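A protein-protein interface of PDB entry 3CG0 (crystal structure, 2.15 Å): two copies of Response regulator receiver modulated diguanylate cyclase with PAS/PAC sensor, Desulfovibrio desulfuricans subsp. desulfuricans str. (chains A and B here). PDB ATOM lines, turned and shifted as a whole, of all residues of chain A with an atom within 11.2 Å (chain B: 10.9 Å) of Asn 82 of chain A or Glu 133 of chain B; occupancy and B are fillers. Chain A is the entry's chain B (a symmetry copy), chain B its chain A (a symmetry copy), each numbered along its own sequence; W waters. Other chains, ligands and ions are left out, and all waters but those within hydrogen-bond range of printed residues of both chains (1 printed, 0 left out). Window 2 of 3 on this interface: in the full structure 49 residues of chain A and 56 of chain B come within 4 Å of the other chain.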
ATOM      1  N   GLY A  11     -15.349  13.878  15.026  1.00  0.00           N
ATOM      2  CA  GLY A  11     -16.730  14.135  15.429  1.00  0.00           C
ATOM      3  C   GLY A  11     -16.877  15.246  16.454  1.00  0.00           C
ATOM      4  O   GLY A  11     -16.171  15.269  17.470  1.00  0.00           O
ATOM      5  N   LEU A  13     -19.500  17.633  18.936  1.00  0.00           N
ATOM      6  CA  LEU A  13     -20.745  17.926  19.648  1.00  0.00           C
ATOM      7  C   LEU A  13     -20.848  19.427  19.936  1.00  0.00           C
ATOM      8  O   LEU A  13     -19.885  20.040  20.412  1.00  0.00           O
ATOM      9  CB  LEU A  13     -20.767  17.155  20.964  1.00  0.00           C
ATOM     10  CG  LEU A  13     -22.102  16.913  21.654  1.00  0.00           C
ATOM     11  CD1 LEU A  13     -22.261  15.456  22.027  1.00  0.00           C
ATOM     12  CD2 LEU A  13     -22.257  17.815  22.882  1.00  0.00           C
ATOM     13  N   ALA A  46     -27.539  16.989  26.211  1.00  0.00           N
ATOM     14  CA  ALA A  46     -26.204  16.912  25.625  1.00  0.00           C
ATOM     15  C   ALA A  46     -25.367  15.872  26.358  1.00  0.00           C
ATOM     16  O   ALA A  46     -24.763  15.018  25.725  1.00  0.00           O
ATOM     17  CB  ALA A  46     -25.510  18.268  25.689  1.00  0.00           C
ATOM     18  N   VAL A  47     -25.349  15.963  27.690  1.00  0.00           N
ATOM     19  CA  VAL A  47     -24.587  15.069  28.565  1.00  0.00           C
ATOM     20  C   VAL A  47     -25.162  13.641  28.538  1.00  0.00           C
ATOM     21  O   VAL A  47     -24.425  12.664  28.658  1.00  0.00           O
ATOM     22  CB  VAL A  47     -24.535  15.635  30.022  1.00  0.00           C
ATOM     23  CG1 VAL A  47     -23.976  14.618  31.018  1.00  0.00           C
ATOM     24  CG2 VAL A  47     -23.708  16.932  30.078  1.00  0.00           C
ATOM     25  N   ALA A  50     -24.420  12.219  24.664  1.00  0.00           N
ATOM     26  CA  ALA A  50     -23.010  12.208  24.264  1.00  0.00           C
ATOM     27  C   ALA A  50     -22.269  10.858  24.303  1.00  0.00           C
ATOM     28  O   ALA A  50     -21.561  10.550  23.344  1.00  0.00           O
ATOM     29  CB  ALA A  50     -22.234  13.262  25.010  1.00  0.00           C
ATOM     30  N   PRO A  51     -22.420  10.051  25.389  1.00  0.00           N
ATOM     31  CA  PRO A  51     -21.740   8.749  25.403  1.00  0.00           C
ATOM     32  C   PRO A  51     -22.082   7.827  24.229  1.00  0.00           C
ATOM     33  O   PRO A  51     -21.182   7.229  23.640  1.00  0.00           O
ATOM     34  CB  PRO A  51     -22.212   8.124  26.720  1.00  0.00           C
ATOM     35  CG  PRO A  51     -22.502   9.281  27.579  1.00  0.00           C
ATOM     36  CD  PRO A  51     -23.154  10.254  26.655  1.00  0.00           C
ATOM     37  N   ASP A  52     -23.359   7.736  23.871  1.00  0.00           N
ATOM     38  CA  ASP A  52     -23.780   6.873  22.764  1.00  0.00           C
ATOM     39  C   ASP A  52     -23.707   7.588  21.403  1.00  0.00           C
ATOM     40  O   ASP A  52     -24.521   7.347  20.506  1.00  0.00           O
ATOM     41  CB  ASP A  52     -25.172   6.268  23.042  1.00  0.00           C
ATOM     42  CG  ASP A  52     -25.110   5.013  23.943  1.00  0.00           C
ATOM     43  OD1 ASP A  52     -24.394   5.032  24.970  1.00  0.00           O
ATOM     44  OD2 ASP A  52     -25.786   4.004  23.624  1.00  0.00           O
ATOM     45  N   LEU A  53     -22.697   8.449  21.266  1.00  0.00           N
ATOM     46  CA  LEU A  53     -22.466   9.267  20.081  1.00  0.00           C
ATOM     47  C   LEU A  53     -20.952   9.344  19.868  1.00  0.00           C
ATOM     48  O   LEU A  53     -20.475   9.460  18.733  1.00  0.00           O
ATOM     49  CB  LEU A  53     -23.037  10.664  20.323  1.00  0.00           C
ATOM     50  CG  LEU A  53     -23.866  11.450  19.314  1.00  0.00           C
ATOM     51  CD1 LEU A  53     -24.764  10.566  18.440  1.00  0.00           C
ATOM     52  CD2 LEU A  53     -24.706  12.454  20.090  1.00  0.00           C
ATOM     53  N   ARG A  54     -20.221   9.267  20.982  1.00  0.00           N
ATOM     54  CA  ARG A  54     -18.754   9.206  21.018  1.00  0.00           C
ATOM     55  C   ARG A  54     -18.048  10.318  20.220  1.00  0.00           C
ATOM     56  O   ARG A  54     -17.318  10.035  19.265  1.00  0.00           O
ATOM     57  CB  ARG A  54     -18.264   7.809  20.588  1.00  0.00           C
ATOM     58  CG  ARG A  54     -18.683   6.673  21.525  1.00  0.00           C
ATOM     59  CD  ARG A  54     -18.763   5.312  20.819  1.00  0.00           C
ATOM     60  NE  ARG A  54     -19.155   4.252  21.753  1.00  0.00           N
ATOM     61  CZ  ARG A  54     -20.386   3.752  21.881  1.00  0.00           C
ATOM     62  NH1 ARG A  54     -21.388   4.187  21.120  1.00  0.00           N
ATOM     63  NH2 ARG A  54     -20.618   2.799  22.774  1.00  0.00           N
ATOM     64  N   PRO A  55     -18.266  11.587  20.603  1.00  0.00           N
ATOM     65  CA  PRO A  55     -17.603  12.647  19.854  1.00  0.00           C
ATOM     66  C   PRO A  55     -16.109  12.805  20.197  1.00  0.00           C
ATOM     67  O   PRO A  55     -15.659  12.345  21.243  1.00  0.00           O
ATOM     68  CB  PRO A  55     -18.395  13.889  20.248  1.00  0.00           C
ATOM     69  CG  PRO A  55     -18.957  13.590  21.565  1.00  0.00           C
ATOM     70  CD  PRO A  55     -19.097  12.123  21.699  1.00  0.00           C
ATOM     71  N   ASP A  56     -15.350  13.433  19.306  1.00  0.00           N
ATOM     72  CA  ASP A  56     -13.940  13.719  19.563  1.00  0.00           C
ATOM     73  C   ASP A  56     -13.739  15.032  20.327  1.00  0.00           C
ATOM     74  O   ASP A  56     -12.746  15.195  21.044  1.00  0.00           O
ATOM     75  CB  ASP A  56     -13.163  13.742  18.248  1.00  0.00           C
ATOM     76  CG  ASP A  56     -13.039  12.362  17.623  1.00  0.00           C
ATOM     77  OD1 ASP A  56     -13.739  12.085  16.622  1.00  0.00           O
ATOM     78  OD2 ASP A  56     -12.249  11.548  18.147  1.00  0.00           O
ATOM     79  N   ILE A  57     -14.684  15.964  20.174  1.00  0.00           N
ATOM     80  CA  ILE A  57     -14.608  17.259  20.843  1.00  0.00           C
ATOM     81  C   ILE A  57     -16.001  17.857  21.127  1.00  0.00           C
ATOM     82  O   ILE A  57     -16.921  17.659  20.345  1.00  0.00           O
ATOM     83  CB  ILE A  57     -13.686  18.229  20.046  1.00  0.00           C
ATOM     84  CG1 ILE A  57     -13.271  19.419  20.907  1.00  0.00           C
ATOM     85  CG2 ILE A  57     -14.306  18.613  18.707  1.00  0.00           C
ATOM     86  CD1 ILE A  57     -12.142  20.189  20.310  1.00  0.00           C
ATOM     87  N   ALA A  58     -16.151  18.553  22.262  1.00  0.00           N
ATOM     88  CA  ALA A  58     -17.360  19.321  22.553  1.00  0.00           C
ATOM     89  C   ALA A  58     -17.146  20.834  22.539  1.00  0.00           C
ATOM     90  O   ALA A  58     -16.227  21.358  23.170  1.00  0.00           O
ATOM     91  CB  ALA A  58     -17.965  18.898  23.868  1.00  0.00           C
ATOM     92  N   LEU A  59     -18.005  21.514  21.787  1.00  0.00           N
ATOM     93  CA  LEU A  59     -18.036  22.968  21.733  1.00  0.00           C
ATOM     94  C   LEU A  59     -19.211  23.440  22.590  1.00  0.00           C
ATOM     95  O   LEU A  59     -20.362  23.140  22.294  1.00  0.00           O
ATOM     96  CB  LEU A  59     -18.188  23.430  20.278  1.00  0.00           C
ATOM     97  CG  LEU A  59     -16.985  23.779  19.385  1.00  0.00           C
ATOM     98  CD1 LEU A  59     -15.812  22.767  19.404  1.00  0.00           C
ATOM     99  CD2 LEU A  59     -17.485  23.997  17.960  1.00  0.00           C
ATOM    100  N   THR A  73     -22.118  21.742  32.330  1.00  0.00           N
ATOM    101  CA  THR A  73     -22.285  20.860  31.169  1.00  0.00           C
ATOM    102  C   THR A  73     -20.932  20.382  30.660  1.00  0.00           C
ATOM    103  O   THR A  73     -20.743  19.181  30.400  1.00  0.00           O
ATOM    104  CB  THR A  73     -23.018  21.572  30.031  1.00  0.00           C
ATOM    105  OG1 THR A  73     -24.290  21.991  30.518  1.00  0.00           O
ATOM    106  CG2 THR A  73     -23.206  20.649  28.804  1.00  0.00           C
ATOM    107  N   ALA A  74     -19.999  21.330  30.545  1.00  0.00           N
ATOM    108  CA  ALA A  74     -18.651  21.049  30.079  1.00  0.00           C
ATOM    109  C   ALA A  74     -17.941  20.128  31.033  1.00  0.00           C
ATOM    110  O   ALA A  74     -17.326  19.172  30.586  1.00  0.00           O
ATOM    111  CB  ALA A  74     -17.881  22.298  29.933  1.00  0.00           C
ATOM    112  N   ALA A  75     -18.049  20.423  32.333  1.00  0.00           N
ATOM    113  CA  ALA A  75     -17.481  19.607  33.419  1.00  0.00           C
ATOM    114  C   ALA A  75     -17.908  18.154  33.318  1.00  0.00           C
ATOM    115  O   ALA A  75     -17.067  17.261  33.362  1.00  0.00           O
ATOM    116  CB  ALA A  75     -17.877  20.178  34.781  1.00  0.00           C
ATOM    117  N   ARG A  76     -19.210  17.941  33.139  1.00  0.00           N
ATOM    118  CA  ARG A  76     -19.760  16.595  33.019  1.00  0.00           C
ATOM    119  C   ARG A  76     -19.465  15.932  31.673  1.00  0.00           C
ATOM    120  O   ARG A  76     -19.436  14.709  31.582  1.00  0.00           O
ATOM    121  CB  ARG A  76     -21.254  16.596  33.330  1.00  0.00           C
ATOM    122  CG  ARG A  76     -21.548  16.862  34.795  1.00  0.00           C
ATOM    123  CD  ARG A  76     -22.951  17.377  34.985  1.00  0.00           C
ATOM    124  NE  ARG A  76     -23.048  18.249  36.154  1.00  0.00           N
ATOM    125  CZ  ARG A  76     -23.781  17.984  37.229  1.00  0.00           C
ATOM    126  NH1 ARG A  76     -23.806  18.852  38.232  1.00  0.00           N
ATOM    127  NH2 ARG A  76     -24.502  16.866  37.293  1.00  0.00           N
ATOM    128  N   LEU A  77     -19.230  16.728  30.636  1.00  0.00           N
ATOM    129  CA  LEU A  77     -18.817  16.173  29.349  1.00  0.00           C
ATOM    130  C   LEU A  77     -17.347  15.751  29.396  1.00  0.00           C
ATOM    131  O   LEU A  77     -16.968  14.719  28.841  1.00  0.00           O
ATOM    132  CB  LEU A  77     -19.039  17.179  28.215  1.00  0.00           C
ATOM    133  CG  LEU A  77     -20.431  17.381  27.613  1.00  0.00           C
ATOM    134  CD1 LEU A  77     -20.436  18.633  26.760  1.00  0.00           C
ATOM    135  CD2 LEU A  77     -20.868  16.185  26.796  1.00  0.00           C
ATOM    136  N   ALA A  78     -16.531  16.561  30.066  1.00  0.00           N
ATOM    137  CA  ALA A  78     -15.102  16.302  30.235  1.00  0.00           C
ATOM    138  C   ALA A  78     -14.817  15.118  31.158  1.00  0.00           C
ATOM    139  O   ALA A  78     -13.848  14.394  30.955  1.00  0.00           O
ATOM    140  CB  ALA A  78     -14.390  17.556  30.742  1.00  0.00           C
ATOM    141  N   ALA A  79     -15.661  14.928  32.169  1.00  0.00           N
ATOM    142  CA  ALA A  79     -15.528  13.805  33.095  1.00  0.00           C
ATOM    143  C   ALA A  79     -16.233  12.549  32.581  1.00  0.00           C
ATOM    144  O   ALA A  79     -15.774  11.433  32.823  1.00  0.00           O
ATOM    145  CB  ALA A  79     -16.055  14.183  34.472  1.00  0.00           C
ATOM    146  N   GLY A  80     -17.341  12.740  31.871  1.00  0.00           N
ATOM    147  CA  GLY A  80     -18.154  11.631  31.382  1.00  0.00           C
ATOM    148  C   GLY A  80     -17.567  10.912  30.186  1.00  0.00           C
ATOM    149  O   GLY A  80     -17.159   9.755  30.294  1.00  0.00           O
ATOM    150  N   CYS A  81     -17.517  11.598  29.047  1.00  0.00           N
ATOM    151  CA  CYS A  81     -17.084  10.984  27.787  1.00  0.00           C
ATOM    152  C   CYS A  81     -15.611  11.247  27.497  1.00  0.00           C
ATOM    153  O   CYS A  81     -15.138  10.975  26.380  1.00  0.00           O
ATOM    154  CB  CYS A  81     -17.937  11.489  26.620  1.00  0.00           C
ATOM    155  SG  CYS A  81     -19.664  11.762  27.026  1.00  0.00           S
ATOM    156  N   ASN A  82     -14.915  11.770  28.515  1.00  0.00           N
ATOM    157  CA  ASN A  82     -13.495  12.133  28.427  1.00  0.00           C
ATOM    158  C   ASN A  82     -13.204  13.025  27.211  1.00  0.00           C
ATOM    159  O   ASN A  82     -12.285  12.769  26.419  1.00  0.00           O
ATOM    160  CB  ASN A  82     -12.600  10.882  28.462  1.00  0.00           C
ATOM    161  CG  ASN A  82     -11.191  11.179  28.939  1.00  0.00           C
ATOM    162  OD1 ASN A  82     -10.973  12.052  29.783  1.00  0.00           O
ATOM    163  ND2 ASN A  82     -10.223  10.449  28.400  1.00  0.00           N
ATOM    164  N   LEU A  83     -14.014  14.070  27.075  1.00  0.00           N
ATOM    165  CA  LEU A  83     -13.936  15.002  25.972  1.00  0.00           C
ATOM    166  C   LEU A  83     -13.088  16.209  26.338  1.00  0.00           C
ATOM    167  O   LEU A  83     -13.180  16.721  27.453  1.00  0.00           O
ATOM    168  CB  LEU A  83     -15.339  15.490  25.602  1.00  0.00           C
ATOM    169  CG  LEU A  83     -16.248  14.636  24.724  1.00  0.00           C
ATOM    170  CD1 LEU A  83     -17.686  15.082  24.859  1.00  0.00           C
ATOM    171  CD2 LEU A  83     -15.817  14.757  23.301  1.00  0.00           C
ATOM    172  N   PRO A  84     -12.260  16.669  25.394  1.00  0.00           N
ATOM    173  CA  PRO A  84     -11.751  18.030  25.508  1.00  0.00           C
ATOM    174  C   PRO A  84     -12.879  19.024  25.169  1.00  0.00           C
ATOM    175  O   PRO A  84     -13.759  18.712  24.356  1.00  0.00           O
ATOM    176  CB  PRO A  84     -10.627  18.068  24.468  1.00  0.00           C
ATOM    177  CG  PRO A  84     -11.034  17.090  23.446  1.00  0.00           C
ATOM    178  CD  PRO A  84     -11.746  15.984  24.196  1.00  0.00           C
ATOM    179  N   ILE A  85     -12.859  20.192  25.812  1.00  0.00           N
ATOM    180  CA  ILE A  85     -13.913  21.181  25.670  1.00  0.00           C
ATOM    181  C   ILE A  85     -13.322  22.497  25.128  1.00  0.00           C
ATOM    182  O   ILE A  85     -12.238  22.903  25.536  1.00  0.00           O
ATOM    183  CB  ILE A  85     -14.690  21.380  27.029  1.00  0.00           C
ATOM    184  CG1 ILE A  85     -16.015  20.611  27.037  1.00  0.00           C
ATOM    185  CG2 ILE A  85     -15.048  22.848  27.293  1.00  0.00           C
ATOM    186  CD1 ILE A  85     -15.904  19.123  27.147  1.00  0.00           C
ATOM    187  N   ILE A  86     -14.007  23.109  24.164  1.00  0.00           N
ATOM    188  CA  ILE A  86     -13.747  24.491  23.789  1.00  0.00           C
ATOM    189  C   ILE A  86     -14.987  25.301  24.149  1.00  0.00           C
ATOM    190  O   ILE A  86     -16.110  24.939  23.776  1.00  0.00           O
ATOM    191  CB  ILE A  86     -13.395  24.623  22.312  1.00  0.00           C
ATOM    192  CG1 ILE A  86     -11.996  24.068  22.060  1.00  0.00           C
ATOM    193  CG2 ILE A  86     -13.463  26.091  21.833  1.00  0.00           C
ATOM    194  CD1 ILE A  86     -11.737  23.772  20.603  1.00  0.00           C
ATOM    195  N   VAL B 103     -12.837  23.414  34.982  1.00  0.00           N
ATOM    196  CA  VAL B 103     -13.052  22.437  33.910  1.00  0.00           C
ATOM    197  C   VAL B 103     -11.728  22.149  33.205  1.00  0.00           C
ATOM    198  O   VAL B 103     -11.520  21.059  32.666  1.00  0.00           O
ATOM    199  CB  VAL B 103     -14.068  22.972  32.858  1.00  0.00           C
ATOM    200  CG1 VAL B 103     -14.201  22.016  31.674  1.00  0.00           C
ATOM    201  CG2 VAL B 103     -15.409  23.224  33.499  1.00  0.00           C
ATOM    202  N   ASN B 104     -10.831  23.135  33.245  1.00  0.00           N
ATOM    203  CA  ASN B 104      -9.646  23.178  32.383  1.00  0.00           C
ATOM    204  C   ASN B 104      -9.987  22.879  30.915  1.00  0.00           C
ATOM    205  O   ASN B 104      -9.673  21.792  30.404  1.00  0.00           O
ATOM    206  CB  ASN B 104      -8.517  22.286  32.923  1.00  0.00           C
ATOM    207  CG  ASN B 104      -8.022  22.736  34.302  1.00  0.00           C
ATOM    208  OD1 ASN B 104      -7.977  21.945  35.247  1.00  0.00           O
ATOM    209  ND2 ASN B 104      -7.652  24.012  34.416  1.00  0.00           N
ATOM    210  N   ALA B 125      -6.670  20.775  19.643  1.00  0.00           N
ATOM    211  CA  ALA B 125      -7.260  20.254  20.878  1.00  0.00           C
ATOM    212  C   ALA B 125      -7.363  18.730  20.914  1.00  0.00           C
ATOM    213  O   ALA B 125      -7.155  18.119  21.969  1.00  0.00           O
ATOM    214  CB  ALA B 125      -8.618  20.861  21.103  1.00  0.00           C
ATOM    215  N   ILE B 126      -7.707  18.133  19.772  1.00  0.00           N
ATOM    216  CA  ILE B 126      -7.855  16.679  19.663  1.00  0.00           C
ATOM    217  C   ILE B 126      -6.486  16.022  19.793  1.00  0.00           C
ATOM    218  O   ILE B 126      -6.302  15.117  20.616  1.00  0.00           O
ATOM    219  CB  ILE B 126      -8.545  16.259  18.329  1.00  0.00           C
ATOM    220  CG1 ILE B 126     -10.011  16.705  18.326  1.00  0.00           C
ATOM    221  CG2 ILE B 126      -8.442  14.738  18.106  1.00  0.00           C
ATOM    222  CD1 ILE B 126     -10.675  16.652  16.960  1.00  0.00           C
ATOM    223  N   HIS B 127      -5.539  16.530  19.000  1.00  0.00           N
ATOM    224  CA  HIS B 127      -4.173  16.021  19.005  1.00  0.00           C
ATOM    225  C   HIS B 127      -3.491  16.172  20.361  1.00  0.00           C
ATOM    226  O   HIS B 127      -2.692  15.320  20.736  1.00  0.00           O
ATOM    227  CB  HIS B 127      -3.357  16.652  17.880  1.00  0.00           C
ATOM    228  CG  HIS B 127      -3.709  16.121  16.526  1.00  0.00           C
ATOM    229  ND1 HIS B 127      -4.825  16.538  15.831  1.00  0.00           N
ATOM    230  CD2 HIS B 127      -3.107  15.192  15.747  1.00  0.00           C
ATOM    231  CE1 HIS B 127      -4.887  15.897  14.677  1.00  0.00           C
ATOM    232  NE2 HIS B 127      -3.857  15.074  14.602  1.00  0.00           N
ATOM    233  N   LYS B 128      -3.845  17.215  21.106  1.00  0.00           N
ATOM    234  CA  LYS B 128      -3.385  17.375  22.472  1.00  0.00           C
ATOM    235  C   LYS B 128      -3.895  16.231  23.341  1.00  0.00           C
ATOM    236  O   LYS B 128      -3.118  15.594  24.041  1.00  0.00           O
ATOM    237  CB  LYS B 128      -3.865  18.705  23.054  1.00  0.00           C
ATOM    238  CG  LYS B 128      -3.174  19.075  24.340  1.00  0.00           C
ATOM    239  CD  LYS B 128      -4.104  19.690  25.354  1.00  0.00           C
ATOM    240  CE  LYS B 128      -3.309  20.086  26.580  1.00  0.00           C
ATOM    241  NZ  LYS B 128      -4.055  20.030  27.871  1.00  0.00           N
ATOM    242  N   LYS B 129      -5.199  15.969  23.255  1.00  0.00           N
ATOM    243  CA  LYS B 129      -5.897  14.978  24.080  1.00  0.00           C
ATOM    244  C   LYS B 129      -5.396  13.554  23.829  1.00  0.00           C
ATOM    245  O   LYS B 129      -5.379  12.725  24.747  1.00  0.00           O
ATOM    246  CB  LYS B 129      -7.415  15.077  23.841  1.00  0.00           C
ATOM    247  CG  LYS B 129      -8.289  14.117  24.655  1.00  0.00           C
ATOM    248  CD  LYS B 129      -8.280  14.436  26.138  1.00  0.00           C
ATOM    249  CE  LYS B 129      -8.994  13.351  26.923  1.00  0.00           C
ATOM    250  NZ  LYS B 129      -9.270  13.776  28.324  1.00  0.00           N
ATOM    251  N   LYS B 130      -4.990  13.296  22.586  1.00  0.00           N
ATOM    252  CA  LYS B 130      -4.356  12.042  22.185  1.00  0.00           C
ATOM    253  C   LYS B 130      -3.113  11.731  23.028  1.00  0.00           C
ATOM    254  O   LYS B 130      -3.003  10.647  23.617  1.00  0.00           O
ATOM    255  CB  LYS B 130      -3.962  12.096  20.703  1.00  0.00           C
ATOM    256  CG  LYS B 130      -5.127  12.041  19.742  1.00  0.00           C
ATOM    257  CD  LYS B 130      -4.669  11.739  18.321  1.00  0.00           C
ATOM    258  CE  LYS B 130      -5.801  11.937  17.310  1.00  0.00           C
ATOM    259  NZ  LYS B 130      -7.044  11.184  17.659  1.00  0.00           N
ATOM    260  N   LEU B 131      -2.202  12.699  23.090  1.00  0.00           N
ATOM    261  CA  LEU B 131      -0.909  12.535  23.748  1.00  0.00           C
ATOM    262  C   LEU B 131      -1.036  12.369  25.259  1.00  0.00           C
ATOM    263  O   LEU B 131      -0.299  11.591  25.861  1.00  0.00           O
ATOM    264  CB  LEU B 131       0.020  13.705  23.402  1.00  0.00           C
ATOM    265  CG  LEU B 131       0.066  14.083  21.918  1.00  0.00           C
ATOM    266  CD1 LEU B 131       0.793  15.396  21.679  1.00  0.00           C
ATOM    267  CD2 LEU B 131       0.659  12.979  21.061  1.00  0.00           C
ATOM    268  N   GLU B 132      -1.996  13.065  25.859  1.00  0.00           N
ATOM    269  CA  GLU B 132      -2.255  12.952  27.294  1.00  0.00           C
ATOM    270  C   GLU B 132      -3.176  11.749  27.579  1.00  0.00           C
ATOM    271  O   GLU B 132      -3.287  10.843  26.741  1.00  0.00           O
ATOM    272  CB  GLU B 132      -2.837  14.272  27.836  1.00  0.00           C
ATOM    273  CG  GLU B 132      -2.188  15.535  27.245  1.00  0.00           C
ATOM    274  CD  GLU B 132      -2.379  16.794  28.085  1.00  0.00           C
ATOM    275  OE1 GLU B 132      -3.440  16.968  28.726  1.00  0.00           O
ATOM    276  OE2 GLU B 132      -1.454  17.629  28.092  1.00  0.00           O
ATOM    277  N   GLU B 133      -3.816  11.733  28.754  1.00  0.00           N
ATOM    278  CA  GLU B 133      -4.779  10.675  29.123  1.00  0.00           C
ATOM    279  C   GLU B 133      -5.995  10.631  28.195  1.00  0.00           C
ATOM    280  O   GLU B 133      -6.689   9.618  28.109  1.00  0.00           O
ATOM    281  CB  GLU B 133      -5.253  10.831  30.576  1.00  0.00           C
ATOM    282  CG  GLU B 133      -4.518   9.955  31.599  1.00  0.00           C
ATOM    283  CD  GLU B 133      -5.308   9.734  32.892  1.00  0.00           C
ATOM    284  OE1 GLU B 133      -6.558   9.796  32.862  1.00  0.00           O
ATOM    285  OE2 GLU B 133      -4.678   9.482  33.944  1.00  0.00           O
HETATM  286  O   HOH W   1     -11.026  20.270  28.181  1.00  0.00           O
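The backbone carbonyl oxygen (O) of Gly 11 of chain A lies within hydrogen-bond range of the backbone NH (N) of Ile 57 of chain A. The backbone NH (N) of Leu 13 of chain A sits at hydrogen-bond distance from the backbone carbonyl oxygen (O) of Ile 57 of chain A, 2.9 Å away. The backbone NH (N) of Ala 58 of chain A lies within hydrogen-bond range of the backbone carbonyl oxygen (O) of Pro 84 of chain A, at 3.2 Å.
No position is printed for both chains. Of the 4 pairs that touch across the chains among the printed residues, none has its exchanged pair printed and touching as well.
Printed residues of chain B within 4 Å of Ile 57 of chain A: Ala 125 (3.7 Å). Ala 78 of chain A touches none of the printed residues of chain B. Cys 81 of chain A touches none of the printed residues of chain B. Printed residues of chain B within 4 Å of Asn 82 of chain A: Lys 129 and Glu 133. No residue of chain B comes within 4 Å of Leu 83 of chain A. Of chain B, only Lys 129 comes within 4 Å of Pro 84 of chain A. Of the printed residues of chain A, Ala 125 of chain B touches Ile 57. Printed residues of chain A within 4 Å of Lys 129 of chain B: Asn 82 (2.8 Å) and Pro 84 (3.96 Å). No residue of chain A comes within 4 Å of Glu 132 of chain B. Of the printed residues of chain A, Glu 133 of chain B touches Asn 82 (3.6 Å). The nearest printed residue of chain B that does not touch Asn 82 of chain A is Glu 132 of chain B (7.1 Å). The nearest printed residue of chain A that does not touch Glu 133 of chain B is Leu 83 of chain A (8.6 Å).
Printed residues of chain A that touch a printed residue of chain B: Ile 57, Asn 82 and Pro 84. Of the 11 printed residues of chain B, 3 touch a printed residue of chain A.
Among the printed residues, pairs that only touch across the chains: Asn 82 of chain A with Glu 133 of chain B, Ile 57 of chain A with Ala 125 of chain B and Pro 84 of chain A with Lys 129 of chain B.
Water W1 lies within hydrogen-bond range of the backbone NH (N) of Ile 85 of chain A (3.0 Å) and the backbone carbonyl oxygen (O) of Asn 104 of chain B (3.0 Å).
The side-chain amide oxygen (OD1) of Asn 82 of chain A is in hydrogen-bond range of the side-chain amino group (NZ) of Lys 129 of chain B, at 2.8 Å.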
